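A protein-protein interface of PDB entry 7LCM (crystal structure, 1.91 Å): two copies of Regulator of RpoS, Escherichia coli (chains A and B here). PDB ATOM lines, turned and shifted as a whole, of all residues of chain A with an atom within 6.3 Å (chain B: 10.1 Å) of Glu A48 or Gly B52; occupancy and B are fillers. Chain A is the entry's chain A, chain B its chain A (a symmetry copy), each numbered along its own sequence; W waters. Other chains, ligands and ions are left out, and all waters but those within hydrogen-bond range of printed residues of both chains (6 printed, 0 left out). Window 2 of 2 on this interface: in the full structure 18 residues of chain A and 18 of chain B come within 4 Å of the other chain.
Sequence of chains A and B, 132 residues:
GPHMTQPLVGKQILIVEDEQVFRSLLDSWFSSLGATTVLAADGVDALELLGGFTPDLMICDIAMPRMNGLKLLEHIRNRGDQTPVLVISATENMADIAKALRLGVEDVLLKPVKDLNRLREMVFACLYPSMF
The side-chain hydroxyl of Thr B36 sits at hydrogen-bond distance from the side-chain carboxylate of Asp A45, at 2.8 Å. OD2 of Asp A45 lies within hydrogen-bond range of NE2 of Gln B12, 3.2 Å away.
N of Ile B13 is in hydrogen-bond range of O of Thr B36 (2.9 Å). The backbone NH (N) of Gln B12 sits at hydrogen-bond distance from the side-chain carboxylate (OD2) of Asp B56, 2.7 Å away. The backbone carbonyl oxygen (O) of Ile B13 sits at hydrogen-bond distance from the backbone NH (N) of Val B38 (2.9 Å).
Among the printed residues, merely in contact across the chains: Glu A48 with Gly B52, Gly A52 with Glu B48, Leu A49 with Phe B53, Glu A48 with Phe B53 and Leu A49 with Val B38.
No residue of chain B comes within 4 Å of Leu A47. No residue of chain B comes within 4 Å of Gly A51. Gly A52 touches one residue of chain B. Printed residues of chain A within 4 Å of Thr B36: Asp A45. Of the printed residues of chain B, Leu A49 touches Val B38 (3.8 Å) and Phe B53 (3.6 Å). Of the printed residues of chain A, Gln B12 touches Asp A45 (3.2 Å). Of the printed residues of chain A, Glu B48 touches Gly A52. Printed residues of chain A within 4 Å of Phe B53: Glu A48 (3.7 Å) and Leu A49 (3.6 Å). Leu A50 touches none of the printed residues of chain B. The nearest printed residue of chain A that does not touch Val B38 is Asp A45 (4.5 Å).
Of the 19 printed residues of chain B, 6 touch a printed residue of chain A. Hydrophobic or aromatic side chains of chain B that line the printed part of chain A: Val B38 and Phe B53. Among the printed residues, 7 pairs touch across the chains. Among the printed residues, no Asp or Glu carboxylate lies within 4 Å of a Lys or Arg side-chain nitrogen of the other chain.
Glu A48 touches Gly B52, and with the chains exchanged Gly A52 touches Glu B48. 8 positions are printed for both chains. Of the 7 pairs that touch across the chains among the printed residues, 2 have their exchanged pair printed and touching as well.
Water W1 bridges OG1 of Thr B54 (2.6 Å) and OE2 of Glu A48 (2.8 Å). Water W6 lies within hydrogen-bond range of O of Gly A52 (2.6 Å) and O of Glu B48 (2.6 Å). Water W3 lies within hydrogen-bond range of the backbone carbonyl oxygen (O) of Gly B52 (2.6 Å) and the backbone carbonyl oxygen (O) of Glu A48 (2.6 Å). Water W4 lies within hydrogen-bond range of the side-chain carboxylate (OE1) of Glu A48 (2.7 Å), the side-chain amide oxygen (OE1) of Gln B12 (2.9 Å) and the backbone NH (N) of Thr B54 (3.0 Å). Water W2 lies within hydrogen-bond range of O of Leu A49, O of Leu B49, N of Gly B52 and N of Gly A52. Water W5 lies within hydrogen-bond range of NE2 of Gln B12, O of Asp A45 and OE1 of Glu A48.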
ATOM      1  N   GLY A  43     -14.009  -8.354 -28.043  1.00  0.00           N
ATOM      2  CA  GLY A  43     -15.194  -8.844 -27.344  1.00  0.00           C
ATOM      3  C   GLY A  43     -14.917  -9.970 -26.357  1.00  0.00           C
ATOM      4  O   GLY A  43     -15.510 -10.016 -25.269  1.00  0.00           O
ATOM      5  N   VAL A  44     -14.059 -10.920 -26.733  1.00  0.00           N
ATOM      6  CA  VAL A  44     -13.659 -11.972 -25.797  1.00  0.00           C
ATOM      7  C   VAL A  44     -12.980 -11.364 -24.575  1.00  0.00           C
ATOM      8  O   VAL A  44     -13.226 -11.778 -23.430  1.00  0.00           O
ATOM      9  CB  VAL A  44     -12.732 -12.978 -26.487  1.00  0.00           C
ATOM     10  CG1 VAL A  44     -12.185 -13.948 -25.451  1.00  0.00           C
ATOM     11  CG2 VAL A  44     -13.475 -13.726 -27.598  1.00  0.00           C
ATOM     12  N   ASP A  45     -12.088 -10.402 -24.802  1.00  0.00           N
ATOM     13  CA  ASP A  45     -11.438  -9.716 -23.677  1.00  0.00           C
ATOM     14  C   ASP A  45     -12.456  -9.023 -22.776  1.00  0.00           C
ATOM     15  O   ASP A  45     -12.356  -9.091 -21.544  1.00  0.00           O
ATOM     16  CB  ASP A  45     -10.415  -8.708 -24.196  1.00  0.00           C
ATOM     17  CG  ASP A  45      -9.108  -9.364 -24.631  1.00  0.00           C
ATOM     18  OD1 ASP A  45      -8.970 -10.610 -24.513  1.00  0.00           O
ATOM     19  OD2 ASP A  45      -8.197  -8.618 -25.056  1.00  0.00           O
ATOM     20  N   ALA A  46     -13.428  -8.329 -23.367  1.00  0.00           N
ATOM     21  CA  ALA A  46     -14.448  -7.650 -22.572  1.00  0.00           C
ATOM     22  C   ALA A  46     -15.256  -8.636 -21.739  1.00  0.00           C
ATOM     23  O   ALA A  46     -15.560  -8.370 -20.567  1.00  0.00           O
ATOM     24  CB  ALA A  46     -15.363  -6.841 -23.488  1.00  0.00           C
ATOM     25  N   LEU A  47     -15.635  -9.768 -22.336  1.00  0.00           N
ATOM     26  CA  LEU A  47     -16.350 -10.816 -21.607  1.00  0.00           C
ATOM     27  C   LEU A  47     -15.590 -11.234 -20.358  1.00  0.00           C
ATOM     28  O   LEU A  47     -16.159 -11.305 -19.265  1.00  0.00           O
ATOM     29  CB  LEU A  47     -16.546 -12.038 -22.506  1.00  0.00           C
ATOM     30  CG  LEU A  47     -17.390 -13.186 -21.931  1.00  0.00           C
ATOM     31  CD1 LEU A  47     -18.561 -12.694 -21.083  1.00  0.00           C
ATOM     32  CD2 LEU A  47     -17.829 -14.167 -23.001  1.00  0.00           C
ATOM     33  N   GLU A  48     -14.302 -11.556 -20.505  1.00  0.00           N
ATOM     34  CA  GLU A  48     -13.538 -11.981 -19.337  1.00  0.00           C
ATOM     35  C   GLU A  48     -13.493 -10.886 -18.274  1.00  0.00           C
ATOM     36  O   GLU A  48     -13.651 -11.173 -17.080  1.00  0.00           O
ATOM     37  CB  GLU A  48     -12.120 -12.366 -19.744  1.00  0.00           C
ATOM     38  CG  GLU A  48     -11.272 -12.854 -18.566  1.00  0.00           C
ATOM     39  CD  GLU A  48      -9.908 -13.333 -19.013  1.00  0.00           C
ATOM     40  OE1 GLU A  48      -9.322 -12.653 -19.863  1.00  0.00           O
ATOM     41  OE2 GLU A  48      -9.431 -14.391 -18.539  1.00  0.00           O
ATOM     42  N   LEU A  49     -13.257  -9.636 -18.690  1.00  0.00           N
ATOM     43  CA  LEU A  49     -13.175  -8.508 -17.754  1.00  0.00           C
ATOM     44  C   LEU A  49     -14.444  -8.369 -16.923  1.00  0.00           C
ATOM     45  O   LEU A  49     -14.380  -8.162 -15.699  1.00  0.00           O
ATOM     46  CB  LEU A  49     -12.936  -7.211 -18.520  1.00  0.00           C
ATOM     47  CG  LEU A  49     -11.569  -6.953 -19.122  1.00  0.00           C
ATOM     48  CD1 LEU A  49     -11.634  -5.644 -19.872  1.00  0.00           C
ATOM     49  CD2 LEU A  49     -10.471  -6.948 -18.036  1.00  0.00           C
ATOM     50  N   LEU A  50     -15.614  -8.490 -17.570  1.00  0.00           N
ATOM     51  CA  LEU A  50     -16.890  -8.332 -16.881  1.00  0.00           C
ATOM     52  C   LEU A  50     -17.086  -9.364 -15.785  1.00  0.00           C
ATOM     53  O   LEU A  50     -17.945  -9.173 -14.917  1.00  0.00           O
ATOM     54  CB  LEU A  50     -18.032  -8.390 -17.900  1.00  0.00           C
ATOM     55  CG  LEU A  50     -18.129  -7.107 -18.726  1.00  0.00           C
ATOM     56  CD1 LEU A  50     -19.008  -7.289 -20.005  1.00  0.00           C
ATOM     57  CD2 LEU A  50     -18.684  -5.988 -17.848  1.00  0.00           C
ATOM     58  N   GLY A  51     -16.316 -10.455 -15.801  1.00  0.00           N
ATOM     59  CA  GLY A  51     -16.328 -11.383 -14.688  1.00  0.00           C
ATOM     60  C   GLY A  51     -15.813 -10.789 -13.388  1.00  0.00           C
ATOM     61  O   GLY A  51     -16.147 -11.293 -12.315  1.00  0.00           O
ATOM     62  N   GLY A  52     -15.016  -9.729 -13.456  1.00  0.00           N
ATOM     63  CA  GLY A  52     -14.406  -9.221 -12.247  1.00  0.00           C
ATOM     64  C   GLY A  52     -14.773  -7.802 -11.866  1.00  0.00           C
ATOM     65  O   GLY A  52     -14.262  -7.300 -10.860  1.00  0.00           O
ATOM     66  N   GLN B  12      -1.918 -10.036 -24.699  1.00  0.00           N
ATOM     67  CA  GLN B  12      -2.853  -9.044 -24.189  1.00  0.00           C
ATOM     68  C   GLN B  12      -2.078  -8.083 -23.298  1.00  0.00           C
ATOM     69  O   GLN B  12      -1.304  -8.531 -22.447  1.00  0.00           O
ATOM     70  CB  GLN B  12      -3.985  -9.724 -23.413  1.00  0.00           C
ATOM     71  CG  GLN B  12      -4.933  -8.753 -22.747  1.00  0.00           C
ATOM     72  CD  GLN B  12      -5.956  -9.450 -21.859  1.00  0.00           C
ATOM     73  OE1 GLN B  12      -5.607 -10.292 -21.031  1.00  0.00           O
ATOM     74  NE2 GLN B  12      -7.224  -9.111 -22.045  1.00  0.00           N
ATOM     75  N   ILE B  13      -2.254  -6.777 -23.508  1.00  0.00           N
ATOM     76  CA  ILE B  13      -1.519  -5.748 -22.776  1.00  0.00           C
ATOM     77  C   ILE B  13      -2.502  -4.877 -22.012  1.00  0.00           C
ATOM     78  O   ILE B  13      -3.407  -4.288 -22.618  1.00  0.00           O
ATOM     79  CB  ILE B  13      -0.689  -4.846 -23.711  1.00  0.00           C
ATOM     80  CG1 ILE B  13       0.180  -5.649 -24.692  1.00  0.00           C
ATOM     81  CG2 ILE B  13       0.130  -3.845 -22.872  1.00  0.00           C
ATOM     82  CD1 ILE B  13       1.101  -6.605 -24.049  1.00  0.00           C
ATOM     83  N   LEU B  14      -2.283  -4.721 -20.702  1.00  0.00           N
ATOM     84  CA  LEU B  14      -3.041  -3.759 -19.900  1.00  0.00           C
ATOM     85  C   LEU B  14      -2.239  -2.469 -19.791  1.00  0.00           C
ATOM     86  O   LEU B  14      -1.068  -2.508 -19.408  1.00  0.00           O
ATOM     87  CB  LEU B  14      -3.325  -4.305 -18.499  1.00  0.00           C
ATOM     88  CG  LEU B  14      -3.833  -3.313 -17.448  1.00  0.00           C
ATOM     89  CD1 LEU B  14      -5.193  -2.753 -17.859  1.00  0.00           C
ATOM     90  CD2 LEU B  14      -3.928  -4.093 -16.128  1.00  0.00           C
ATOM     91  N   THR B  36      -3.778  -7.205 -28.280  1.00  0.00           N
ATOM     92  CA  THR B  36      -5.079  -6.707 -27.854  1.00  0.00           C
ATOM     93  C   THR B  36      -4.869  -5.953 -26.548  1.00  0.00           C
ATOM     94  O   THR B  36      -4.147  -6.422 -25.657  1.00  0.00           O
ATOM     95  CB  THR B  36      -6.106  -7.831 -27.695  1.00  0.00           C
ATOM     96  OG1 THR B  36      -5.792  -8.635 -26.558  1.00  0.00           O
ATOM     97  CG2 THR B  36      -6.054  -8.727 -28.925  1.00  0.00           C
ATOM     98  N   VAL B  38      -6.151  -3.561 -23.191  1.00  0.00           N
ATOM     99  CA  VAL B  38      -7.152  -3.137 -22.225  1.00  0.00           C
ATOM    100  C   VAL B  38      -6.589  -1.883 -21.579  1.00  0.00           C
ATOM    101  O   VAL B  38      -5.425  -1.879 -21.177  1.00  0.00           O
ATOM    102  CB  VAL B  38      -7.424  -4.231 -21.177  1.00  0.00           C
ATOM    103  CG1 VAL B  38      -8.338  -3.689 -20.082  1.00  0.00           C
ATOM    104  CG2 VAL B  38      -8.050  -5.459 -21.847  1.00  0.00           C
ATOM    105  N   ASP B  45      -9.376   1.433 -10.555  1.00  0.00           N
ATOM    106  CA  ASP B  45     -10.064   0.633 -11.579  1.00  0.00           C
ATOM    107  C   ASP B  45      -9.194  -0.521 -12.067  1.00  0.00           C
ATOM    108  O   ASP B  45      -9.679  -1.649 -12.234  1.00  0.00           O
ATOM    109  CB  ASP B  45     -10.475   1.521 -12.751  1.00  0.00           C
ATOM    110  CG  ASP B  45     -11.729   2.338 -12.460  1.00  0.00           C
ATOM    111  OD1 ASP B  45     -12.312   2.208 -11.350  1.00  0.00           O
ATOM    112  OD2 ASP B  45     -12.160   3.086 -13.368  1.00  0.00           O
ATOM    113  N   ALA B  46      -7.914  -0.260 -12.330  1.00  0.00           N
ATOM    114  CA  ALA B  46      -7.016  -1.317 -12.788  1.00  0.00           C
ATOM    115  C   ALA B  46      -6.883  -2.426 -11.752  1.00  0.00           C
ATOM    116  O   ALA B  46      -6.876  -3.616 -12.100  1.00  0.00           O
ATOM    117  CB  ALA B  46      -5.649  -0.724 -13.121  1.00  0.00           C
ATOM    118  N   LEU B  47      -6.748  -2.054 -10.478  1.00  0.00           N
ATOM    119  CA  LEU B  47      -6.688  -3.035  -9.395  1.00  0.00           C
ATOM    120  C   LEU B  47      -7.884  -3.973  -9.435  1.00  0.00           C
ATOM    121  O   LEU B  47      -7.732  -5.196  -9.373  1.00  0.00           O
ATOM    122  CB  LEU B  47      -6.655  -2.323  -8.042  1.00  0.00           C
ATOM    123  CG  LEU B  47      -6.467  -3.210  -6.802  1.00  0.00           C
ATOM    124  CD1 LEU B  47      -5.514  -4.378  -7.048  1.00  0.00           C
ATOM    125  CD2 LEU B  47      -6.085  -2.405  -5.574  1.00  0.00           C
ATOM    126  N   GLU B  48      -9.096  -3.415  -9.498  1.00  0.00           N
ATOM    127  CA  GLU B  48     -10.274  -4.275  -9.520  1.00  0.00           C
ATOM    128  C   GLU B  48     -10.265  -5.201 -10.735  1.00  0.00           C
ATOM    129  O   GLU B  48     -10.583  -6.390 -10.611  1.00  0.00           O
ATOM    130  CB  GLU B  48     -11.545  -3.432  -9.521  1.00  0.00           C
ATOM    131  CG  GLU B  48     -12.822  -4.277  -9.510  1.00  0.00           C
ATOM    132  CD  GLU B  48     -14.064  -3.420  -9.402  1.00  0.00           C
ATOM    133  OE1 GLU B  48     -14.098  -2.387 -10.079  1.00  0.00           O
ATOM    134  OE2 GLU B  48     -14.991  -3.759  -8.629  1.00  0.00           O
ATOM    135  N   LEU B  49      -9.924  -4.664 -11.912  1.00  0.00           N
ATOM    136  CA  LEU B  49      -9.898  -5.456 -13.149  1.00  0.00           C
ATOM    137  C   LEU B  49      -8.972  -6.660 -13.030  1.00  0.00           C
ATOM    138  O   LEU B  49      -9.330  -7.776 -13.441  1.00  0.00           O
ATOM    139  CB  LEU B  49      -9.439  -4.586 -14.314  1.00  0.00           C
ATOM    140  CG  LEU B  49     -10.387  -3.543 -14.872  1.00  0.00           C
ATOM    141  CD1 LEU B  49      -9.658  -2.792 -15.961  1.00  0.00           C
ATOM    142  CD2 LEU B  49     -11.692  -4.191 -15.386  1.00  0.00           C
ATOM    143  N   LEU B  50      -7.776  -6.454 -12.457  1.00  0.00           N
ATOM    144  CA  LEU B  50      -6.794  -7.527 -12.332  1.00  0.00           C
ATOM    145  C   LEU B  50      -7.301  -8.677 -11.481  1.00  0.00           C
ATOM    146  O   LEU B  50      -6.734  -9.774 -11.541  1.00  0.00           O
ATOM    147  CB  LEU B  50      -5.488  -6.960 -11.765  1.00  0.00           C
ATOM    148  CG  LEU B  50      -4.716  -6.149 -12.807  1.00  0.00           C
ATOM    149  CD1 LEU B  50      -3.608  -5.256 -12.164  1.00  0.00           C
ATOM    150  CD2 LEU B  50      -4.108  -7.103 -13.832  1.00  0.00           C
ATOM    151  N   GLY B  51      -8.353  -8.458 -10.686  1.00  0.00           N
ATOM    152  CA  GLY B  51      -8.993  -9.557  -9.991  1.00  0.00           C
ATOM    153  C   GLY B  51      -9.644 -10.572 -10.916  1.00  0.00           C
ATOM    154  O   GLY B  51      -9.843 -11.719 -10.515  1.00  0.00           O
ATOM    155  N   GLY B  52      -9.974 -10.181 -12.142  1.00  0.00           N
ATOM    156  CA  GLY B  52     -10.710 -11.082 -12.999  1.00  0.00           C
ATOM    157  C   GLY B  52     -10.017 -11.490 -14.283  1.00  0.00           C
ATOM    158  O   GLY B  52     -10.607 -12.235 -15.072  1.00  0.00           O
ATOM    159  N   PHE B  53      -8.789 -11.031 -14.522  1.00  0.00           N
ATOM    160  CA  PHE B  53      -8.095 -11.415 -15.749  1.00  0.00           C
ATOM    161  C   PHE B  53      -6.597 -11.371 -15.513  1.00  0.00           C
ATOM    162  O   PHE B  53      -6.113 -10.947 -14.454  1.00  0.00           O
ATOM    163  CB  PHE B  53      -8.541 -10.555 -16.960  1.00  0.00           C
ATOM    164  CG  PHE B  53      -7.794  -9.235 -17.150  1.00  0.00           C
ATOM    165  CD1 PHE B  53      -7.695  -8.296 -16.130  1.00  0.00           C
ATOM    166  CD2 PHE B  53      -7.264  -8.911 -18.395  1.00  0.00           C
ATOM    167  CE1 PHE B  53      -7.054  -7.094 -16.340  1.00  0.00           C
ATOM    168  CE2 PHE B  53      -6.616  -7.715 -18.614  1.00  0.00           C
ATOM    169  CZ  PHE B  53      -6.504  -6.798 -17.579  1.00  0.00           C
ATOM    170  N   THR B  54      -5.863 -11.845 -16.515  1.00  0.00           N
ATOM    171  CA  THR B  54      -4.430 -12.095 -16.391  1.00  0.00           C
ATOM    172  C   THR B  54      -3.768 -11.590 -17.661  1.00  0.00           C
ATOM    173  O   THR B  54      -3.507 -12.367 -18.585  1.00  0.00           O
ATOM    174  CB  THR B  54      -4.140 -13.592 -16.200  1.00  0.00           C
ATOM    175  OG1 THR B  54      -4.834 -14.357 -17.204  1.00  0.00           O
ATOM    176  CG2 THR B  54      -4.635 -14.069 -14.854  1.00  0.00           C
ATOM    177  N   PRO B  55      -3.483 -10.289 -17.753  1.00  0.00           N
ATOM    178  CA  PRO B  55      -2.775  -9.776 -18.932  1.00  0.00           C
ATOM    179  C   PRO B  55      -1.361 -10.339 -19.015  1.00  0.00           C
ATOM    180  O   PRO B  55      -0.777 -10.786 -18.027  1.00  0.00           O
ATOM    181  CB  PRO B  55      -2.758  -8.259 -18.717  1.00  0.00           C
ATOM    182  CG  PRO B  55      -2.863  -8.087 -17.227  1.00  0.00           C
ATOM    183  CD  PRO B  55      -3.751  -9.231 -16.764  1.00  0.00           C
ATOM    184  N   ASP B  56      -0.811 -10.335 -20.232  1.00  0.00           N
ATOM    185  CA  ASP B  56       0.555 -10.804 -20.426  1.00  0.00           C
ATOM    186  C   ASP B  56       1.571  -9.776 -19.961  1.00  0.00           C
ATOM    187  O   ASP B  56       2.691 -10.137 -19.577  1.00  0.00           O
ATOM    188  CB  ASP B  56       0.760 -11.119 -21.889  1.00  0.00           C
ATOM    189  CG  ASP B  56      -0.088 -12.276 -22.320  1.00  0.00           C
ATOM    190  OD1 ASP B  56       0.089 -13.369 -21.749  1.00  0.00           O
ATOM    191  OD2 ASP B  56      -0.982 -12.073 -23.161  1.00  0.00           O
ATOM    192  N   ILE B  76      -0.904  -5.441  -5.928  1.00  0.00           N
ATOM    193  CA  ILE B  76      -0.995  -6.676  -6.692  1.00  0.00           C
ATOM    194  C   ILE B  76       0.202  -7.572  -6.405  1.00  0.00           C
ATOM    195  O   ILE B  76       0.069  -8.799  -6.406  1.00  0.00           O
ATOM    196  CB  ILE B  76      -1.195  -6.387  -8.186  1.00  0.00           C
ATOM    197  CG1 ILE B  76      -0.021  -5.660  -8.814  1.00  0.00           C
ATOM    198  CG2 ILE B  76      -2.431  -5.515  -8.371  1.00  0.00           C
ATOM    199  CD1 ILE B  76      -0.324  -5.240 -10.272  1.00  0.00           C
ATOM    200  N   ASP B  81       0.578 -11.619  -7.321  1.00  0.00           N
ATOM    201  CA  ASP B  81       0.549 -11.407  -8.766  1.00  0.00           C
ATOM    202  C   ASP B  81       1.959 -11.121  -9.276  1.00  0.00           C
ATOM    203  O   ASP B  81       2.589 -10.147  -8.850  1.00  0.00           O
ATOM    204  CB  ASP B  81      -0.396 -10.250  -9.082  1.00  0.00           C
ATOM    205  CG  ASP B  81      -0.615 -10.042 -10.574  1.00  0.00           C
ATOM    206  OD1 ASP B  81       0.373  -9.808 -11.290  1.00  0.00           O
ATOM    207  OD2 ASP B  81      -1.782 -10.057 -11.023  1.00  0.00           O
HETATM  208  O   HOH W   1      -7.279 -15.044 -16.949  1.00  0.00           O
HETATM  209  O   HOH W   2     -12.021  -8.484 -14.111  1.00  0.00           O
HETATM  210  O   HOH W   3     -13.095 -12.853 -15.145  1.00  0.00           O
HETATM  211  O   HOH W   4      -6.652 -12.461 -19.373  1.00  0.00           O
HETATM  212  O   HOH W   5      -9.672  -9.846 -20.674  1.00  0.00           O
HETATM  213  O   HOH W   6     -12.234  -8.109  -9.515  1.00  0.00           O
